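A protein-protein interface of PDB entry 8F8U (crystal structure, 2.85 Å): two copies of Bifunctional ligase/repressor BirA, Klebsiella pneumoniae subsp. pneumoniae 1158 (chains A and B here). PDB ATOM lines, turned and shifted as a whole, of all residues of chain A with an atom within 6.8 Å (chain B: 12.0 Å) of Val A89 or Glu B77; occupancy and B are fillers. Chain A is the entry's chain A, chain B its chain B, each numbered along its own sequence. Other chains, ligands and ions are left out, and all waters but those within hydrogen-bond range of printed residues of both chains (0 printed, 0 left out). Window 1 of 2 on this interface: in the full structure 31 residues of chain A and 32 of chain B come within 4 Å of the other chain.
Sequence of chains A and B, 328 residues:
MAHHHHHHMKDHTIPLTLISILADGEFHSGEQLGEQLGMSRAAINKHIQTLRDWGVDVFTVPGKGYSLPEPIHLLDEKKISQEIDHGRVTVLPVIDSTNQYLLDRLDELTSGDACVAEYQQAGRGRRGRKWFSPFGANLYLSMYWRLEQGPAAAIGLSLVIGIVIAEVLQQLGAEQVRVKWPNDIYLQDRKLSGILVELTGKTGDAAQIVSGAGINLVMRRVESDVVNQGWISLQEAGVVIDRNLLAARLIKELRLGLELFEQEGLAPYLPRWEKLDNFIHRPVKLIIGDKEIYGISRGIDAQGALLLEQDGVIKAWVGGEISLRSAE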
ATOM      1  N   GLY A  87      -9.592  20.058 -23.233  1.00  0.00           N
ATOM      2  CA  GLY A  87      -9.061  18.874 -23.879  1.00  0.00           C
ATOM      3  C   GLY A  87      -8.091  18.082 -23.025  1.00  0.00           C
ATOM      4  O   GLY A  87      -7.479  18.625 -22.100  1.00  0.00           O
ATOM      5  N   ARG A  88      -7.941  16.797 -23.329  1.00  0.00           N
ATOM      6  CA  ARG A  88      -7.045  15.912 -22.605  1.00  0.00           C
ATOM      7  C   ARG A  88      -5.746  15.721 -23.385  1.00  0.00           C
ATOM      8  O   ARG A  88      -5.595  16.189 -24.514  1.00  0.00           O
ATOM      9  CB  ARG A  88      -7.715  14.560 -22.344  1.00  0.00           C
ATOM     10  CG  ARG A  88      -9.157  14.658 -21.875  1.00  0.00           C
ATOM     11  CD  ARG A  88      -9.938  13.400 -22.223  1.00  0.00           C
ATOM     12  NE  ARG A  88     -10.912  13.636 -23.281  1.00  0.00           N
ATOM     13  CZ  ARG A  88     -11.698  12.702 -23.800  1.00  0.00           C
ATOM     14  NH1 ARG A  88     -11.661  11.451 -23.369  1.00  0.00           N
ATOM     15  NH2 ARG A  88     -12.547  13.033 -24.768  1.00  0.00           N
ATOM     16  N   VAL A  89      -4.800  15.024 -22.758  1.00  0.00           N
ATOM     17  CA  VAL A  89      -3.517  14.706 -23.380  1.00  0.00           C
ATOM     18  C   VAL A  89      -3.188  13.249 -23.084  1.00  0.00           C
ATOM     19  O   VAL A  89      -3.062  12.864 -21.916  1.00  0.00           O
ATOM     20  CB  VAL A  89      -2.380  15.616 -22.882  1.00  0.00           C
ATOM     21  CG1 VAL A  89      -1.049  15.151 -23.450  1.00  0.00           C
ATOM     22  CG2 VAL A  89      -2.643  17.065 -23.258  1.00  0.00           C
ATOM     23  N   THR A  90      -3.050  12.444 -24.132  1.00  0.00           N
ATOM     24  CA  THR A  90      -2.565  11.074 -24.016  1.00  0.00           C
ATOM     25  C   THR A  90      -1.166  11.018 -24.609  1.00  0.00           C
ATOM     26  O   THR A  90      -0.972  11.360 -25.781  1.00  0.00           O
ATOM     27  CB  THR A  90      -3.498  10.091 -24.724  1.00  0.00           C
ATOM     28  OG1 THR A  90      -3.276  10.148 -26.139  1.00  0.00           O
ATOM     29  CG2 THR A  90      -4.951  10.428 -24.429  1.00  0.00           C
ATOM     30  N   VAL A  91      -0.215  10.599 -23.764  1.00  0.00           N
ATOM     31  CA  VAL A  91       1.219  10.546 -24.165  1.00  0.00           C
ATOM     32  C   VAL A  91       1.660   9.096 -24.303  1.00  0.00           C
ATOM     33  O   VAL A  91       1.610   8.367 -23.305  1.00  0.00           O
ATOM     34  CB  VAL A  91       2.105  11.265 -23.134  1.00  0.00           C
ATOM     35  CG1 VAL A  91       3.582  11.088 -23.444  1.00  0.00           C
ATOM     36  CG2 VAL A  91       1.752  12.738 -23.009  1.00  0.00           C
ATOM     37  N   GLY A 112      -9.384  20.157 -28.666  1.00  0.00           N
ATOM     38  CA  GLY A 112      -8.282  20.346 -27.754  1.00  0.00           C
ATOM     39  C   GLY A 112      -7.591  19.067 -27.324  1.00  0.00           C
ATOM     40  O   GLY A 112      -6.471  19.135 -26.803  1.00  0.00           O
ATOM     41  N   ASP A 113      -8.229  17.912 -27.518  1.00  0.00           N
ATOM     42  CA  ASP A 113      -7.590  16.642 -27.195  1.00  0.00           C
ATOM     43  C   ASP A 113      -6.303  16.487 -27.991  1.00  0.00           C
ATOM     44  O   ASP A 113      -6.264  16.758 -29.195  1.00  0.00           O
ATOM     45  CB  ASP A 113      -8.533  15.477 -27.493  1.00  0.00           C
ATOM     46  CG  ASP A 113      -9.570  15.269 -26.408  1.00  0.00           C
ATOM     47  OD1 ASP A 113      -9.431  15.878 -25.327  1.00  0.00           O
ATOM     48  OD2 ASP A 113     -10.521  14.492 -26.638  1.00  0.00           O
ATOM     49  N   ALA A 114      -5.246  16.034 -27.321  1.00  0.00           N
ATOM     50  CA  ALA A 114      -3.920  15.998 -27.915  1.00  0.00           C
ATOM     51  C   ALA A 114      -3.246  14.660 -27.650  1.00  0.00           C
ATOM     52  O   ALA A 114      -3.584  13.943 -26.705  1.00  0.00           O
ATOM     53  CB  ALA A 114      -3.041  17.141 -27.384  1.00  0.00           C
ATOM     54  N   CYS A 115      -2.279  14.337 -28.506  1.00  0.00           N
ATOM     55  CA  CYS A 115      -1.494  13.113 -28.392  1.00  0.00           C
ATOM     56  C   CYS A 115      -0.035  13.451 -28.656  1.00  0.00           C
ATOM     57  O   CYS A 115       0.279  14.097 -29.663  1.00  0.00           O
ATOM     58  CB  CYS A 115      -1.986  12.041 -29.372  1.00  0.00           C
ATOM     59  SG  CYS A 115      -0.835  10.672 -29.633  1.00  0.00           S
ATOM     60  N   VAL A 116       0.850  13.010 -27.766  1.00  0.00           N
ATOM     61  CA  VAL A 116       2.255  13.405 -27.775  1.00  0.00           C
ATOM     62  C   VAL A 116       3.130  12.161 -27.829  1.00  0.00           C
ATOM     63  O   VAL A 116       2.830  11.152 -27.183  1.00  0.00           O
ATOM     64  CB  VAL A 116       2.612  14.258 -26.539  1.00  0.00           C
ATOM     65  CG1 VAL A 116       3.854  15.087 -26.813  1.00  0.00           C
ATOM     66  CG2 VAL A 116       1.444  15.148 -26.149  1.00  0.00           C
ATOM     67  N   LEU A 141       3.313  15.672 -32.155  1.00  0.00           N
ATOM     68  CA  LEU A 141       2.157  16.209 -31.454  1.00  0.00           C
ATOM     69  C   LEU A 141       1.003  16.324 -32.435  1.00  0.00           C
ATOM     70  O   LEU A 141       1.190  16.800 -33.557  1.00  0.00           O
ATOM     71  CB  LEU A 141       2.469  17.579 -30.838  1.00  0.00           C
ATOM     72  CG  LEU A 141       1.337  18.313 -30.116  1.00  0.00           C
ATOM     73  CD1 LEU A 141       0.602  17.385 -29.158  1.00  0.00           C
ATOM     74  CD2 LEU A 141       1.876  19.530 -29.383  1.00  0.00           C
ATOM     75  N   ASN A 244       9.159  17.843 -22.434  1.00  0.00           N
ATOM     76  CA  ASN A 244       7.879  18.037 -21.766  1.00  0.00           C
ATOM     77  C   ASN A 244       7.478  19.505 -21.773  1.00  0.00           C
ATOM     78  O   ASN A 244       6.303  19.837 -21.971  1.00  0.00           O
ATOM     79  CB  ASN A 244       7.941  17.505 -20.337  1.00  0.00           C
ATOM     80  CG  ASN A 244       8.157  16.007 -20.284  1.00  0.00           C
ATOM     81  OD1 ASN A 244       7.379  15.238 -20.844  1.00  0.00           O
ATOM     82  ND2 ASN A 244       9.221  15.587 -19.608  1.00  0.00           N
ATOM     83  N   ILE A 251       0.744  22.584 -26.712  1.00  0.00           N
ATOM     84  CA  ILE A 251      -0.655  22.187 -26.524  1.00  0.00           C
ATOM     85  C   ILE A 251      -1.453  23.335 -25.916  1.00  0.00           C
ATOM     86  O   ILE A 251      -2.592  23.605 -26.318  1.00  0.00           O
ATOM     87  CB  ILE A 251      -0.746  20.916 -25.654  1.00  0.00           C
ATOM     88  CG1 ILE A 251       0.243  19.854 -26.134  1.00  0.00           C
ATOM     89  CG2 ILE A 251      -2.160  20.357 -25.663  1.00  0.00           C
ATOM     90  CD1 ILE A 251      -0.075  18.448 -25.673  1.00  0.00           C
ATOM     91  N   ARG A 255      -4.099  25.258 -28.345  1.00  0.00           N
ATOM     92  CA  ARG A 255      -5.493  25.298 -27.922  1.00  0.00           C
ATOM     93  C   ARG A 255      -6.023  26.724 -27.966  1.00  0.00           C
ATOM     94  O   ARG A 255      -7.079  26.986 -28.553  1.00  0.00           O
ATOM     95  CB  ARG A 255      -5.637  24.717 -26.516  1.00  0.00           C
ATOM     96  CG  ARG A 255      -5.846  23.214 -26.475  1.00  0.00           C
ATOM     97  CD  ARG A 255      -5.673  22.682 -25.063  1.00  0.00           C
ATOM     98  NE  ARG A 255      -5.550  21.230 -25.031  1.00  0.00           N
ATOM     99  CZ  ARG A 255      -5.128  20.540 -23.983  1.00  0.00           C
ATOM    100  NH1 ARG A 255      -4.778  21.138 -22.855  1.00  0.00           N
ATOM    101  NH2 ARG A 255      -5.051  19.214 -24.066  1.00  0.00           N
ATOM    102  N   LEU B  16      10.049   0.523 -22.662  1.00  0.00           N
ATOM    103  CA  LEU B  16      10.038   1.871 -22.099  1.00  0.00           C
ATOM    104  C   LEU B  16      10.463   1.867 -20.635  1.00  0.00           C
ATOM    105  O   LEU B  16      11.244   2.729 -20.209  1.00  0.00           O
ATOM    106  CB  LEU B  16       8.657   2.504 -22.257  1.00  0.00           C
ATOM    107  CG  LEU B  16       8.328   3.069 -23.640  1.00  0.00           C
ATOM    108  CD1 LEU B  16       6.874   3.506 -23.702  1.00  0.00           C
ATOM    109  CD2 LEU B  16       9.257   4.224 -23.993  1.00  0.00           C
ATOM    110  N   HIS B  73      15.422  11.902 -21.242  1.00  0.00           N
ATOM    111  CA  HIS B  73      14.202  12.386 -20.618  1.00  0.00           C
ATOM    112  C   HIS B  73      13.026  11.949 -21.477  1.00  0.00           C
ATOM    113  O   HIS B  73      12.998  12.215 -22.683  1.00  0.00           O
ATOM    114  CB  HIS B  73      14.226  13.908 -20.474  1.00  0.00           C
ATOM    115  CG  HIS B  73      15.188  14.400 -19.440  1.00  0.00           C
ATOM    116  ND1 HIS B  73      15.637  13.613 -18.402  1.00  0.00           N
ATOM    117  CD2 HIS B  73      15.794  15.602 -19.288  1.00  0.00           C
ATOM    118  CE1 HIS B  73      16.477  14.307 -17.654  1.00  0.00           C
ATOM    119  NE2 HIS B  73      16.588  15.517 -18.170  1.00  0.00           N
ATOM    120  N   LEU B  74      12.064  11.283 -20.856  1.00  0.00           N
ATOM    121  CA  LEU B  74      10.932  10.731 -21.580  1.00  0.00           C
ATOM    122  C   LEU B  74       9.713  11.613 -21.375  1.00  0.00           C
ATOM    123  O   LEU B  74       9.586  12.308 -20.363  1.00  0.00           O
ATOM    124  CB  LEU B  74      10.632   9.305 -21.115  1.00  0.00           C
ATOM    125  CG  LEU B  74      10.952   8.170 -22.090  1.00  0.00           C
ATOM    126  CD1 LEU B  74      12.455   7.978 -22.219  1.00  0.00           C
ATOM    127  CD2 LEU B  74      10.282   6.884 -21.639  1.00  0.00           C
ATOM    128  N   LEU B  75       8.807  11.573 -22.345  1.00  0.00           N
ATOM    129  CA  LEU B  75       7.552  12.293 -22.209  1.00  0.00           C
ATOM    130  C   LEU B  75       6.712  11.649 -21.119  1.00  0.00           C
ATOM    131  O   LEU B  75       6.461  10.440 -21.139  1.00  0.00           O
ATOM    132  CB  LEU B  75       6.804  12.312 -23.536  1.00  0.00           C
ATOM    133  CG  LEU B  75       7.494  13.097 -24.653  1.00  0.00           C
ATOM    134  CD1 LEU B  75       7.054  12.582 -26.004  1.00  0.00           C
ATOM    135  CD2 LEU B  75       7.211  14.584 -24.523  1.00  0.00           C
ATOM    136  N   ASP B  76       6.285  12.462 -20.159  1.00  0.00           N
ATOM    137  CA  ASP B  76       5.448  12.013 -19.056  1.00  0.00           C
ATOM    138  C   ASP B  76       4.214  12.894 -18.993  1.00  0.00           C
ATOM    139  O   ASP B  76       4.325  14.125 -19.038  1.00  0.00           O
ATOM    140  CB  ASP B  76       6.206  12.059 -17.726  1.00  0.00           C
ATOM    141  CG  ASP B  76       5.723  11.009 -16.744  1.00  0.00           C
ATOM    142  OD1 ASP B  76       4.512  10.701 -16.752  1.00  0.00           O
ATOM    143  OD2 ASP B  76       6.553  10.491 -15.966  1.00  0.00           O
ATOM    144  N   GLU B  77       3.040  12.266 -18.917  1.00  0.00           N
ATOM    145  CA  GLU B  77       1.800  13.021 -18.765  1.00  0.00           C
ATOM    146  C   GLU B  77       1.873  13.938 -17.553  1.00  0.00           C
ATOM    147  O   GLU B  77       1.493  15.112 -17.621  1.00  0.00           O
ATOM    148  CB  GLU B  77       0.613  12.062 -18.642  1.00  0.00           C
ATOM    149  CG  GLU B  77      -0.532  12.584 -17.788  1.00  0.00           C
ATOM    150  CD  GLU B  77      -1.888  12.122 -18.276  1.00  0.00           C
ATOM    151  OE1 GLU B  77      -1.968  11.018 -18.858  1.00  0.00           O
ATOM    152  OE2 GLU B  77      -2.876  12.859 -18.073  1.00  0.00           O
ATOM    153  N   LYS B  78       2.371  13.412 -16.432  1.00  0.00           N
ATOM    154  CA  LYS B  78       2.407  14.192 -15.201  1.00  0.00           C
ATOM    155  C   LYS B  78       3.348  15.384 -15.334  1.00  0.00           C
ATOM    156  O   LYS B  78       3.009  16.498 -14.918  1.00  0.00           O
ATOM    157  CB  LYS B  78       2.820  13.305 -14.020  1.00  0.00           C
ATOM    158  CG  LYS B  78       2.038  11.990 -13.855  1.00  0.00           C
ATOM    159  CD  LYS B  78       0.621  12.048 -14.426  1.00  0.00           C
ATOM    160  CE  LYS B  78      -0.190  10.817 -14.065  1.00  0.00           C
ATOM    161  NZ  LYS B  78      -1.550  11.186 -13.589  1.00  0.00           N
ATOM    162  N   LYS B  79       4.534  15.167 -15.909  1.00  0.00           N
ATOM    163  CA  LYS B  79       5.455  16.275 -16.146  1.00  0.00           C
ATOM    164  C   LYS B  79       4.845  17.300 -17.096  1.00  0.00           C
ATOM    165  O   LYS B  79       4.923  18.511 -16.855  1.00  0.00           O
ATOM    166  CB  LYS B  79       6.777  15.751 -16.710  1.00  0.00           C
ATOM    167  CG  LYS B  79       7.803  15.365 -15.659  1.00  0.00           C
ATOM    168  CD  LYS B  79       9.216  15.655 -16.144  1.00  0.00           C
ATOM    169  CE  LYS B  79       9.665  17.051 -15.750  1.00  0.00           C
ATOM    170  NZ  LYS B  79      11.027  17.043 -15.148  1.00  0.00           N
ATOM    171  N   ILE B  80       4.233  16.828 -18.183  1.00  0.00           N
ATOM    172  CA  ILE B  80       3.662  17.739 -19.165  1.00  0.00           C
ATOM    173  C   ILE B  80       2.501  18.520 -18.561  1.00  0.00           C
ATOM    174  O   ILE B  80       2.501  19.756 -18.564  1.00  0.00           O
ATOM    175  CB  ILE B  80       3.239  16.963 -20.429  1.00  0.00           C
ATOM    176  CG1 ILE B  80       4.422  16.820 -21.389  1.00  0.00           C
ATOM    177  CG2 ILE B  80       2.098  17.652 -21.144  1.00  0.00           C
ATOM    178  CD1 ILE B  80       4.388  15.550 -22.211  1.00  0.00           C
ATOM    179  N   SER B  81       1.545  17.812 -17.949  1.00  0.00           N
ATOM    180  CA  SER B  81       0.321  18.454 -17.469  1.00  0.00           C
ATOM    181  C   SER B  81       0.612  19.494 -16.396  1.00  0.00           C
ATOM    182  O   SER B  81      -0.164  20.441 -16.225  1.00  0.00           O
ATOM    183  CB  SER B  81      -0.657  17.408 -16.937  1.00  0.00           C
ATOM    184  OG  SER B  81      -0.837  16.357 -17.867  1.00  0.00           O
ATOM    185  N   GLN B  82       1.707  19.326 -15.667  1.00  0.00           N
ATOM    186  CA  GLN B  82       2.060  20.343 -14.651  1.00  0.00           C
ATOM    187  C   GLN B  82       2.222  21.695 -15.342  1.00  0.00           C
ATOM    188  O   GLN B  82       1.701  22.687 -14.810  1.00  0.00           O
ATOM    189  CB  GLN B  82       3.340  19.945 -13.926  1.00  0.00           C
ATOM    190  CG  GLN B  82       3.578  20.722 -12.641  1.00  0.00           C
ATOM    191  CD  GLN B  82       2.342  20.806 -11.781  1.00  0.00           C
ATOM    192  OE1 GLN B  82       1.926  21.884 -11.367  1.00  0.00           O
ATOM    193  NE2 GLN B  82       1.747  19.658 -11.498  1.00  0.00           N
ATOM    194  N   GLU B  83       2.897  21.725 -16.490  1.00  0.00           N
ATOM    195  CA  GLU B  83       3.180  22.997 -17.145  1.00  0.00           C
ATOM    196  C   GLU B  83       1.948  23.628 -17.795  1.00  0.00           C
ATOM    197  O   GLU B  83       1.877  24.859 -17.892  1.00  0.00           O
ATOM    198  CB  GLU B  83       4.302  22.806 -18.171  1.00  0.00           C
ATOM    199  CG  GLU B  83       4.622  24.022 -19.036  1.00  0.00           C
ATOM    200  CD  GLU B  83       5.189  25.190 -18.245  1.00  0.00           C
ATOM    201  OE1 GLU B  83       5.744  24.966 -17.147  1.00  0.00           O
ATOM    202  OE2 GLU B  83       5.083  26.337 -18.731  1.00  0.00           O
ATOM    203  N   ILE B  84       0.963  22.838 -18.234  1.00  0.00           N
ATOM    204  CA  ILE B  84      -0.228  23.465 -18.811  1.00  0.00           C
ATOM    205  C   ILE B  84      -1.112  24.058 -17.722  1.00  0.00           C
ATOM    206  O   ILE B  84      -1.644  25.163 -17.871  1.00  0.00           O
ATOM    207  CB  ILE B  84      -1.047  22.506 -19.704  1.00  0.00           C
ATOM    208  CG1 ILE B  84      -0.227  21.860 -20.817  1.00  0.00           C
ATOM    209  CG2 ILE B  84      -2.241  23.220 -20.316  1.00  0.00           C
ATOM    210  CD1 ILE B  84       0.372  20.587 -20.424  1.00  0.00           C
ATOM    211  N   ASP B  85      -1.278  23.345 -16.609  1.00  0.00           N
ATOM    212  CA  ASP B  85      -2.285  23.710 -15.624  1.00  0.00           C
ATOM    213  C   ASP B  85      -1.729  24.431 -14.405  1.00  0.00           C
ATOM    214  O   ASP B  85      -2.485  25.138 -13.732  1.00  0.00           O
ATOM    215  CB  ASP B  85      -3.044  22.464 -15.156  1.00  0.00           C
ATOM    216  CG  ASP B  85      -3.705  21.729 -16.300  1.00  0.00           C
ATOM    217  OD1 ASP B  85      -4.114  22.395 -17.271  1.00  0.00           O
ATOM    218  OD2 ASP B  85      -3.812  20.486 -16.227  1.00  0.00           O
ATOM    219  N   HIS B  86      -0.440  24.270 -14.104  1.00  0.00           N
ATOM    220  CA  HIS B  86       0.159  24.805 -12.881  1.00  0.00           C
ATOM    221  C   HIS B  86      -0.576  24.264 -11.649  1.00  0.00           C
ATOM    222  O   HIS B  86      -1.178  25.003 -10.869  1.00  0.00           O
ATOM    223  CB  HIS B  86       0.175  26.337 -12.900  1.00  0.00           C
ATOM    224  CG  HIS B  86       1.272  26.941 -12.077  1.00  0.00           C
ATOM    225  ND1 HIS B  86       2.005  28.029 -12.501  1.00  0.00           N
ATOM    226  CD2 HIS B  86       1.756  26.614 -10.857  1.00  0.00           C
ATOM    227  CE1 HIS B  86       2.899  28.341 -11.579  1.00  0.00           C
ATOM    228  NE2 HIS B  86       2.768  27.499 -10.570  1.00  0.00           N
ATOM    229  N   GLY B  87      -0.513  22.945 -11.494  1.00  0.00           N
ATOM    230  CA  GLY B  87      -1.133  22.272 -10.370  1.00  0.00           C
ATOM    231  C   GLY B  87      -2.151  21.230 -10.785  1.00  0.00           C
ATOM    232  O   GLY B  87      -2.699  21.299 -11.889  1.00  0.00           O
ATOM    233  N   ARG B  88      -2.413  20.263  -9.912  1.00  0.00           N
ATOM    234  CA  ARG B  88      -3.370  19.203 -10.182  1.00  0.00           C
ATOM    235  C   ARG B  88      -4.695  19.483  -9.480  1.00  0.00           C
ATOM    236  O   ARG B  88      -4.831  20.431  -8.702  1.00  0.00           O
ATOM    237  CB  ARG B  88      -2.810  17.848  -9.742  1.00  0.00           C
ATOM    238  CG  ARG B  88      -1.447  17.523 -10.327  1.00  0.00           C
ATOM    239  CD  ARG B  88      -0.814  16.346  -9.610  1.00  0.00           C
ATOM    240  NE  ARG B  88       0.381  16.741  -8.876  1.00  0.00           N
ATOM    241  CZ  ARG B  88       0.613  16.440  -7.606  1.00  0.00           C
ATOM    242  NH1 ARG B  88      -0.248  15.730  -6.894  1.00  0.00           N
ATOM    243  NH2 ARG B  88       1.736  16.863  -7.032  1.00  0.00           N
ATOM    244  N   VAL B  89      -5.682  18.639  -9.770  1.00  0.00           N
ATOM    245  CA  VAL B  89      -7.004  18.729  -9.156  1.00  0.00           C
ATOM    246  C   VAL B  89      -7.429  17.329  -8.740  1.00  0.00           C
ATOM    247  O   VAL B  89      -7.548  16.436  -9.586  1.00  0.00           O
ATOM    248  CB  VAL B  89      -8.059  19.338 -10.100  1.00  0.00           C
ATOM    249  CG1 VAL B  89      -9.271  19.800  -9.304  1.00  0.00           C
ATOM    250  CG2 VAL B  89      -7.478  20.488 -10.911  1.00  0.00           C
ATOM    251  N   THR B 110       2.488  21.031  -4.877  1.00  0.00           N
ATOM    252  CA  THR B 110       3.110  22.096  -5.647  1.00  0.00           C
ATOM    253  C   THR B 110       2.087  23.208  -5.828  1.00  0.00           C
ATOM    254  O   THR B 110       0.878  22.958  -5.828  1.00  0.00           O
ATOM    255  CB  THR B 110       3.612  21.600  -7.011  1.00  0.00           C
ATOM    256  OG1 THR B 110       4.025  22.718  -7.809  1.00  0.00           O
ATOM    257  CG2 THR B 110       2.520  20.837  -7.739  1.00  0.00           C
ATOM    258  N   ASP B 113      -1.933  23.183  -6.773  1.00  0.00           N
ATOM    259  CA  ASP B 113      -2.659  21.951  -6.498  1.00  0.00           C
ATOM    260  C   ASP B 113      -3.952  22.260  -5.757  1.00  0.00           C
ATOM    261  O   ASP B 113      -3.971  23.063  -4.821  1.00  0.00           O
ATOM    262  CB  ASP B 113      -1.795  20.993  -5.673  1.00  0.00           C
ATOM    263  CG  ASP B 113      -0.770  20.257  -6.512  1.00  0.00           C
ATOM    264  OD1 ASP B 113      -0.907  20.241  -7.753  1.00  0.00           O
ATOM    265  OD2 ASP B 113       0.172  19.686  -5.925  1.00  0.00           O
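The backbone NH of Lys B78 sits close to the side-chain carboxylate of Asp B76, 3.5 Å away. The side-chain hydroxyl of Ser B81 is in hydrogen-bond range of the backbone carbonyl oxygen of Glu B77 (2.7 Å).
4 positions are printed for both chains. Of the 8 pairs that touch across the chains among the printed residues, none has its exchanged pair printed and touching as well.
Val A89 touches Glu B77 (O to OE1, 3.7 Å). CB of Leu B75 touches CG1 of Val A91, at 3.4 Å. CD1 of Ile B80 touches CG2 of Val A91 (3.9 Å). OD1 of Asn A244 touches CA of Leu B75, at 3.3 Å. ND2 of Asn A244 touches CD of Lys B79, 3.5 Å away. Ile B80 touches Asn A244.
No residue of chain B comes within 4 Å of Gly A87. Of chain B, only Glu B77 (3.7 Å) comes within 4 Å of Val A89. No residue of chain B comes within 4 Å of Thr A90. Asp A113 touches none of the printed residues of chain B. No residue of chain B comes within 4 Å of Ala A114. No residue of chain B comes within 4 Å of Val A116. Of the printed residues of chain B, Asn A244 touches Leu B74 (3.4 Å), Leu B75 (3.3 Å), Asp B76 (3.1 Å), Lys B79 (3.5 Å) and Ile B80 (3.3 Å). No residue of chain B comes within 4 Å of Ile A251. Printed residues of chain A within 4 Å of Lys B79: Asn A244 (3.5 Å). Of the printed residues of chain A, Ile B80 touches Val A91 (3.9 Å) and Asn A244 (3.3 Å). The nearest residue of chain B that does not touch Val A89 is Ile B80 (4.6 Å).
Of the 14 printed residues of chain A, 3 touch a printed residue of chain B. Hydrophobic or aromatic side chains of chain A that line the printed part of chain B: Val A91. Hydrophobic or aromatic side chains of chain B that line the printed part of chain A: Leu B75 and Ile B80.
The backbone carbonyl oxygen (O) of Leu B74 sits at hydrogen-bond distance from the side-chain amide nitrogen (ND2) of Asn A244 (3.4 Å). The side-chain amide oxygen of Asn A244 sits at hydrogen-bond distance from the backbone NH of Asp B76, 3.1 Å away.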
